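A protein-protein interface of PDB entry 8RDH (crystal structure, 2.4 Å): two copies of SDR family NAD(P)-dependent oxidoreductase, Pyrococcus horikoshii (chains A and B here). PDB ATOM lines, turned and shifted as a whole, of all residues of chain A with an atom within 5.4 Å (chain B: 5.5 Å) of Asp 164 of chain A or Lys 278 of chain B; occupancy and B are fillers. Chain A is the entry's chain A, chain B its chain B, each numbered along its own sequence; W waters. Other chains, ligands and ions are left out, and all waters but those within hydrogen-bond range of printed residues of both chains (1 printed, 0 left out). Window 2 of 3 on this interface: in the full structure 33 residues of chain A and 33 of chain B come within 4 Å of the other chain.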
ATOM      1  N   TYR A 159     -20.669  -4.600  16.130  1.00  0.00           N
ATOM      2  CA  TYR A 159     -21.516  -3.642  15.426  1.00  0.00           C
ATOM      3  C   TYR A 159     -22.214  -4.287  14.237  1.00  0.00           C
ATOM      4  O   TYR A 159     -23.380  -3.988  13.959  1.00  0.00           O
ATOM      5  CB  TYR A 159     -20.684  -2.445  14.971  1.00  0.00           C
ATOM      6  CG  TYR A 159     -20.675  -1.292  15.942  1.00  0.00           C
ATOM      7  CD1 TYR A 159     -19.970  -1.361  17.133  1.00  0.00           C
ATOM      8  CD2 TYR A 159     -21.356  -0.116  15.649  1.00  0.00           C
ATOM      9  CE1 TYR A 159     -19.960  -0.301  18.016  1.00  0.00           C
ATOM     10  CE2 TYR A 159     -21.349   0.947  16.521  1.00  0.00           C
ATOM     11  CZ  TYR A 159     -20.649   0.851  17.702  1.00  0.00           C
ATOM     12  OH  TYR A 159     -20.638   1.909  18.574  1.00  0.00           O
ATOM     13  N   ALA A 160     -21.512  -5.160  13.509  1.00  0.00           N
ATOM     14  CA  ALA A 160     -22.127  -5.847  12.380  1.00  0.00           C
ATOM     15  C   ALA A 160     -23.350  -6.631  12.824  1.00  0.00           C
ATOM     16  O   ALA A 160     -24.384  -6.622  12.147  1.00  0.00           O
ATOM     17  CB  ALA A 160     -21.113  -6.776  11.716  1.00  0.00           C
ATOM     18  N   HIS A 161     -23.247  -7.325  13.957  1.00  0.00           N
ATOM     19  CA  HIS A 161     -24.388  -8.111  14.417  1.00  0.00           C
ATOM     20  C   HIS A 161     -25.485  -7.238  15.016  1.00  0.00           C
ATOM     21  O   HIS A 161     -26.670  -7.472  14.754  1.00  0.00           O
ATOM     22  CB  HIS A 161     -23.932  -9.153  15.431  1.00  0.00           C
ATOM     23  CG  HIS A 161     -23.337 -10.369  14.802  1.00  0.00           C
ATOM     24  ND1 HIS A 161     -21.980 -10.536  14.639  1.00  0.00           N
ATOM     25  CD2 HIS A 161     -23.920 -11.469  14.273  1.00  0.00           C
ATOM     26  CE1 HIS A 161     -21.750 -11.694  14.047  1.00  0.00           C
ATOM     27  NE2 HIS A 161     -22.910 -12.279  13.811  1.00  0.00           N
ATOM     28  N   THR A 162     -25.125  -6.236  15.822  1.00  0.00           N
ATOM     29  CA  THR A 162     -26.148  -5.427  16.480  1.00  0.00           C
ATOM     30  C   THR A 162     -26.906  -4.561  15.481  1.00  0.00           C
ATOM     31  O   THR A 162     -28.109  -4.330  15.645  1.00  0.00           O
ATOM     32  CB  THR A 162     -25.516  -4.552  17.565  1.00  0.00           C
ATOM     33  OG1 THR A 162     -24.938  -5.380  18.579  1.00  0.00           O
ATOM     34  CG2 THR A 162     -26.557  -3.636  18.196  1.00  0.00           C
ATOM     35  N   PHE A 163     -26.225  -4.066  14.445  1.00  0.00           N
ATOM     36  CA  PHE A 163     -26.796  -3.067  13.552  1.00  0.00           C
ATOM     37  C   PHE A 163     -26.953  -3.565  12.122  1.00  0.00           C
ATOM     38  O   PHE A 163     -27.207  -2.760  11.219  1.00  0.00           O
ATOM     39  CB  PHE A 163     -25.937  -1.800  13.593  1.00  0.00           C
ATOM     40  CG  PHE A 163     -25.801  -1.224  14.973  1.00  0.00           C
ATOM     41  CD1 PHE A 163     -26.889  -0.645  15.599  1.00  0.00           C
ATOM     42  CD2 PHE A 163     -24.594  -1.274  15.650  1.00  0.00           C
ATOM     43  CE1 PHE A 163     -26.777  -0.122  16.875  1.00  0.00           C
ATOM     44  CE2 PHE A 163     -24.475  -0.747  16.922  1.00  0.00           C
ATOM     45  CZ  PHE A 163     -25.569  -0.170  17.533  1.00  0.00           C
ATOM     46  N   ASP A 164     -26.819  -4.869  11.893  1.00  0.00           N
ATOM     47  CA  ASP A 164     -27.264  -5.512  10.659  1.00  0.00           C
ATOM     48  C   ASP A 164     -26.596  -4.912   9.421  1.00  0.00           C
ATOM     49  O   ASP A 164     -27.245  -4.373   8.525  1.00  0.00           O
ATOM     50  CB  ASP A 164     -28.789  -5.451  10.545  1.00  0.00           C
ATOM     51  CG  ASP A 164     -29.478  -6.310  11.581  1.00  0.00           C
ATOM     52  OD1 ASP A 164     -28.786  -7.134  12.217  1.00  0.00           O
ATOM     53  OD2 ASP A 164     -30.706  -6.166  11.761  1.00  0.00           O
ATOM     54  N   PHE A 165     -25.275  -5.024   9.389  1.00  0.00           N
ATOM     55  CA  PHE A 165     -24.504  -4.940   8.159  1.00  0.00           C
ATOM     56  C   PHE A 165     -23.503  -6.086   8.161  1.00  0.00           C
ATOM     57  O   PHE A 165     -23.355  -6.804   9.154  1.00  0.00           O
ATOM     58  CB  PHE A 165     -23.804  -3.585   8.008  1.00  0.00           C
ATOM     59  CG  PHE A 165     -22.854  -3.256   9.117  1.00  0.00           C
ATOM     60  CD1 PHE A 165     -21.534  -3.673   9.068  1.00  0.00           C
ATOM     61  CD2 PHE A 165     -23.276  -2.509  10.199  1.00  0.00           C
ATOM     62  CE1 PHE A 165     -20.658  -3.359  10.088  1.00  0.00           C
ATOM     63  CE2 PHE A 165     -22.405  -2.190  11.220  1.00  0.00           C
ATOM     64  CZ  PHE A 165     -21.096  -2.617  11.166  1.00  0.00           C
ATOM     65  N   ARG A 166     -22.819  -6.269   7.039  1.00  0.00           N
ATOM     66  CA  ARG A 166     -21.913  -7.394   6.860  1.00  0.00           C
ATOM     67  C   ARG A 166     -20.472  -6.912   6.860  1.00  0.00           C
ATOM     68  O   ARG A 166     -20.165  -5.841   6.329  1.00  0.00           O
ATOM     69  CB  ARG A 166     -22.226  -8.142   5.563  1.00  0.00           C
ATOM     70  CG  ARG A 166     -23.610  -8.780   5.568  1.00  0.00           C
ATOM     71  CD  ARG A 166     -23.876  -9.584   4.314  1.00  0.00           C
ATOM     72  NE  ARG A 166     -22.974 -10.724   4.200  1.00  0.00           N
ATOM     73  CZ  ARG A 166     -22.514 -11.209   3.054  1.00  0.00           C
ATOM     74  NH1 ARG A 166     -22.841 -10.669   1.892  1.00  0.00           N
ATOM     75  NH2 ARG A 166     -21.700 -12.260   3.078  1.00  0.00           N
ATOM     76  N   ARG A 234     -22.433 -13.240   8.017  1.00  0.00           N
ATOM     77  CA  ARG A 234     -22.542 -11.899   8.585  1.00  0.00           C
ATOM     78  C   ARG A 234     -21.166 -11.288   8.821  1.00  0.00           C
ATOM     79  O   ARG A 234     -20.950 -10.102   8.550  1.00  0.00           O
ATOM     80  CB  ARG A 234     -23.341 -11.976   9.890  1.00  0.00           C
ATOM     81  CG  ARG A 234     -23.310 -10.738  10.783  1.00  0.00           C
ATOM     82  CD  ARG A 234     -24.164  -9.615  10.246  1.00  0.00           C
ATOM     83  NE  ARG A 234     -25.544 -10.026  10.017  1.00  0.00           N
ATOM     84  CZ  ARG A 234     -26.457  -9.268   9.426  1.00  0.00           C
ATOM     85  NH1 ARG A 234     -26.181  -8.038   9.025  1.00  0.00           N
ATOM     86  NH2 ARG A 234     -27.678  -9.757   9.233  1.00  0.00           N
ATOM     87  N   VAL B  82     -25.578  -5.678  28.597  1.00  0.00           N
ATOM     88  CA  VAL B  82     -25.630  -6.043  27.181  1.00  0.00           C
ATOM     89  C   VAL B  82     -26.786  -5.340  26.483  1.00  0.00           C
ATOM     90  O   VAL B  82     -26.643  -4.836  25.361  1.00  0.00           O
ATOM     91  CB  VAL B  82     -25.746  -7.573  27.032  1.00  0.00           C
ATOM     92  CG1 VAL B  82     -25.980  -7.959  25.571  1.00  0.00           C
ATOM     93  CG2 VAL B  82     -24.508  -8.252  27.560  1.00  0.00           C
ATOM     94  N   ARG B  83     -27.948  -5.296  27.140  1.00  0.00           N
ATOM     95  CA  ARG B  83     -29.178  -4.865  26.482  1.00  0.00           C
ATOM     96  C   ARG B  83     -29.057  -3.476  25.869  1.00  0.00           C
ATOM     97  O   ARG B  83     -29.711  -3.189  24.860  1.00  0.00           O
ATOM     98  CB  ARG B  83     -30.332  -4.881  27.486  1.00  0.00           C
ATOM     99  CG  ARG B  83     -31.669  -4.357  26.949  1.00  0.00           C
ATOM    100  CD  ARG B  83     -32.726  -4.339  28.048  1.00  0.00           C
ATOM    101  NE  ARG B  83     -32.150  -3.915  29.319  1.00  0.00           N
ATOM    102  CZ  ARG B  83     -32.160  -4.622  30.442  1.00  0.00           C
ATOM    103  NH1 ARG B  83     -32.869  -5.733  30.560  1.00  0.00           N
ATOM    104  NH2 ARG B  83     -31.469  -4.179  31.488  1.00  0.00           N
ATOM    105  N   SER B  86     -27.683  -1.894  21.623  1.00  0.00           N
ATOM    106  CA  SER B  86     -28.352  -1.457  20.401  1.00  0.00           C
ATOM    107  C   SER B  86     -28.775   0.006  20.474  1.00  0.00           C
ATOM    108  O   SER B  86     -28.901   0.661  19.433  1.00  0.00           O
ATOM    109  CB  SER B  86     -29.562  -2.349  20.117  1.00  0.00           C
ATOM    110  OG  SER B  86     -30.527  -2.270  21.151  1.00  0.00           O
ATOM    111  N   ILE B 142     -21.404 -10.904  19.029  1.00  0.00           N
ATOM    112  CA  ILE B 142     -22.599 -10.423  18.349  1.00  0.00           C
ATOM    113  C   ILE B 142     -23.181  -9.180  19.004  1.00  0.00           C
ATOM    114  O   ILE B 142     -24.161  -8.621  18.492  1.00  0.00           O
ATOM    115  CB  ILE B 142     -23.678 -11.525  18.275  1.00  0.00           C
ATOM    116  CG1 ILE B 142     -24.251 -11.827  19.666  1.00  0.00           C
ATOM    117  CG2 ILE B 142     -23.096 -12.788  17.678  1.00  0.00           C
ATOM    118  CD1 ILE B 142     -25.446 -12.744  19.647  1.00  0.00           C
ATOM    119  N   SER B 143     -22.609  -8.725  20.113  1.00  0.00           N
ATOM    120  CA  SER B 143     -23.100  -7.560  20.828  1.00  0.00           C
ATOM    121  C   SER B 143     -21.995  -6.524  20.954  1.00  0.00           C
ATOM    122  O   SER B 143     -20.804  -6.842  20.920  1.00  0.00           O
ATOM    123  CB  SER B 143     -23.615  -7.941  22.224  1.00  0.00           C
ATOM    124  OG  SER B 143     -22.567  -8.450  23.030  1.00  0.00           O
ATOM    125  N   VAL B 271     -36.544 -11.208  19.713  1.00  0.00           N
ATOM    126  CA  VAL B 271     -36.093 -10.696  18.428  1.00  0.00           C
ATOM    127  C   VAL B 271     -34.999 -11.621  17.929  1.00  0.00           C
ATOM    128  O   VAL B 271     -34.428 -12.403  18.692  1.00  0.00           O
ATOM    129  CB  VAL B 271     -35.525  -9.261  18.525  1.00  0.00           C
ATOM    130  CG1 VAL B 271     -36.479  -8.343  19.268  1.00  0.00           C
ATOM    131  CG2 VAL B 271     -34.144  -9.289  19.180  1.00  0.00           C
ATOM    132  N   ASP B 272     -34.694 -11.521  16.637  1.00  0.00           N
ATOM    133  CA  ASP B 272     -33.518 -12.192  16.087  1.00  0.00           C
ATOM    134  C   ASP B 272     -33.487 -13.670  16.466  1.00  0.00           C
ATOM    135  O   ASP B 272     -32.418 -14.263  16.626  1.00  0.00           O
ATOM    136  CB  ASP B 272     -32.250 -11.471  16.561  1.00  0.00           C
ATOM    137  CG  ASP B 272     -31.007 -11.890  15.803  1.00  0.00           C
ATOM    138  OD1 ASP B 272     -31.087 -12.068  14.570  1.00  0.00           O
ATOM    139  OD2 ASP B 272     -29.940 -12.010  16.442  1.00  0.00           O
ATOM    140  N   GLY B 276     -33.615 -12.206  23.890  1.00  0.00           N
ATOM    141  CA  GLY B 276     -34.211 -11.188  24.737  1.00  0.00           C
ATOM    142  C   GLY B 276     -34.067  -9.790  24.171  1.00  0.00           C
ATOM    143  O   GLY B 276     -34.905  -8.922  24.430  1.00  0.00           O
ATOM    144  N   TRP B 277     -33.018  -9.557  23.389  1.00  0.00           N
ATOM    145  CA  TRP B 277     -32.694  -8.255  22.820  1.00  0.00           C
ATOM    146  C   TRP B 277     -31.591  -8.493  21.799  1.00  0.00           C
ATOM    147  O   TRP B 277     -30.980  -9.565  21.763  1.00  0.00           O
ATOM    148  CB  TRP B 277     -32.249  -7.247  23.886  1.00  0.00           C
ATOM    149  CG  TRP B 277     -31.238  -7.818  24.831  1.00  0.00           C
ATOM    150  CD1 TRP B 277     -29.924  -8.087  24.567  1.00  0.00           C
ATOM    151  CD2 TRP B 277     -31.459  -8.203  26.193  1.00  0.00           C
ATOM    152  NE1 TRP B 277     -29.317  -8.618  25.679  1.00  0.00           N
ATOM    153  CE2 TRP B 277     -30.238  -8.698  26.691  1.00  0.00           C
ATOM    154  CE3 TRP B 277     -32.572  -8.177  27.040  1.00  0.00           C
ATOM    155  CZ2 TRP B 277     -30.097  -9.161  27.996  1.00  0.00           C
ATOM    156  CZ3 TRP B 277     -32.428  -8.637  28.338  1.00  0.00           C
ATOM    157  CH2 TRP B 277     -31.201  -9.123  28.801  1.00  0.00           C
ATOM    158  N   LYS B 278     -31.348  -7.489  20.963  1.00  0.00           N
ATOM    159  CA  LYS B 278     -30.283  -7.605  19.978  1.00  0.00           C
ATOM    160  C   LYS B 278     -28.951  -7.847  20.676  1.00  0.00           C
ATOM    161  O   LYS B 278     -28.538  -7.067  21.540  1.00  0.00           O
ATOM    162  CB  LYS B 278     -30.220  -6.349  19.108  1.00  0.00           C
ATOM    163  CG  LYS B 278     -29.610  -6.593  17.730  1.00  0.00           C
ATOM    164  CD  LYS B 278     -30.436  -7.577  16.897  1.00  0.00           C
ATOM    165  CE  LYS B 278     -29.654  -8.096  15.705  1.00  0.00           C
ATOM    166  NZ  LYS B 278     -29.493  -7.056  14.656  1.00  0.00           N
ATOM    167  N   GLY B 279     -28.280  -8.933  20.300  1.00  0.00           N
ATOM    168  CA  GLY B 279     -27.014  -9.302  20.888  1.00  0.00           C
ATOM    169  C   GLY B 279     -27.100 -10.304  22.022  1.00  0.00           C
ATOM    170  O   GLY B 279     -26.056 -10.803  22.461  1.00  0.00           O
ATOM    171  N   ASP B 280     -28.303 -10.619  22.506  1.00  0.00           N
ATOM    172  CA  ASP B 280     -28.459 -11.607  23.571  1.00  0.00           C
ATOM    173  C   ASP B 280     -28.104 -12.980  23.018  1.00  0.00           C
ATOM    174  O   ASP B 280     -28.827 -13.520  22.176  1.00  0.00           O
ATOM    175  CB  ASP B 280     -29.884 -11.596  24.117  1.00  0.00           C
ATOM    176  CG  ASP B 280     -30.112 -12.651  25.193  1.00  0.00           C
ATOM    177  OD1 ASP B 280     -29.215 -12.845  26.042  1.00  0.00           O
ATOM    178  OD2 ASP B 280     -31.195 -13.276  25.198  1.00  0.00           O
HETATM  179  O   HOH W   1     -25.827  -5.270  21.186  1.00  0.00           O
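Ile 142 of chain B touches His 161 of chain A (O to CB, 3.1 Å).
Thr 162 of chain A touches Ser 86 of chain B (CG2 to CA, 3.6 Å).
OG1 of Thr 162 of chain A touches CA of Ser 143 of chain B, at 3.6 Å.
Phe 163 of chain A touches Ser 86 of chain B.
Water W1 lies within hydrogen-bond range of the side-chain hydroxyl of Thr 162 of chain A (2.8 Å) and the backbone carbonyl oxygen of Lys 278 of chain B (3.3 Å).
Hydrophobic or aromatic side chains of chain B within 4 Å of the printed part of chain A: Ile 142.
Among the printed residues, 8 pairs touch across the chains.
The backbone carbonyl oxygen (O) of His 161 of chain A is in hydrogen-bond range of the side-chain amino group (NZ) of Lys 278 of chain B (2.9 Å).
O of Ile 142 of chain B is in hydrogen-bond range of OG1 of Thr 162 of chain A, at 3.3 Å.
The backbone carbonyl oxygen (O) of Thr 162 of chain A sits at hydrogen-bond distance from the side-chain amino group (NZ) of Lys 278 of chain B, at 3.2 Å.
The side-chain amino group of Lys 278 of chain B is in salt-bridge range of the side-chain carboxylate of Asp 164 of chain A.
Asp 164 of chain A touches just one residue of chain B: Lys 278.
Of chain A, only His 161 (2.9 Å), Thr 162 (3.2 Å) and Asp 164 (2.5 Å) come within 4 Å of Lys 278 of chain B.
Of the printed residues of chain A, Ser 143 of chain B touches Thr 162.
Of the printed residues of chain B, His 161 of chain A touches Ile 142 (3.1 Å) and Lys 278 (2.9 Å).
Of the printed residues of chain A, Ile 142 of chain B touches His 161 (3.1 Å) and Thr 162 (3.3 Å).
The nearest printed residue of chain B that does not touch Asp 164 of chain A is Asp 272 of chain B (5.9 Å).
The nearest residue of chain A that does not touch Lys 278 of chain B is Phe 163 of chain A (4.4 Å).
The nearest printed residue of chain A that does not touch Ile 142 of chain B is Tyr 159 of chain A (5.8 Å).
No position is printed for both chains.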
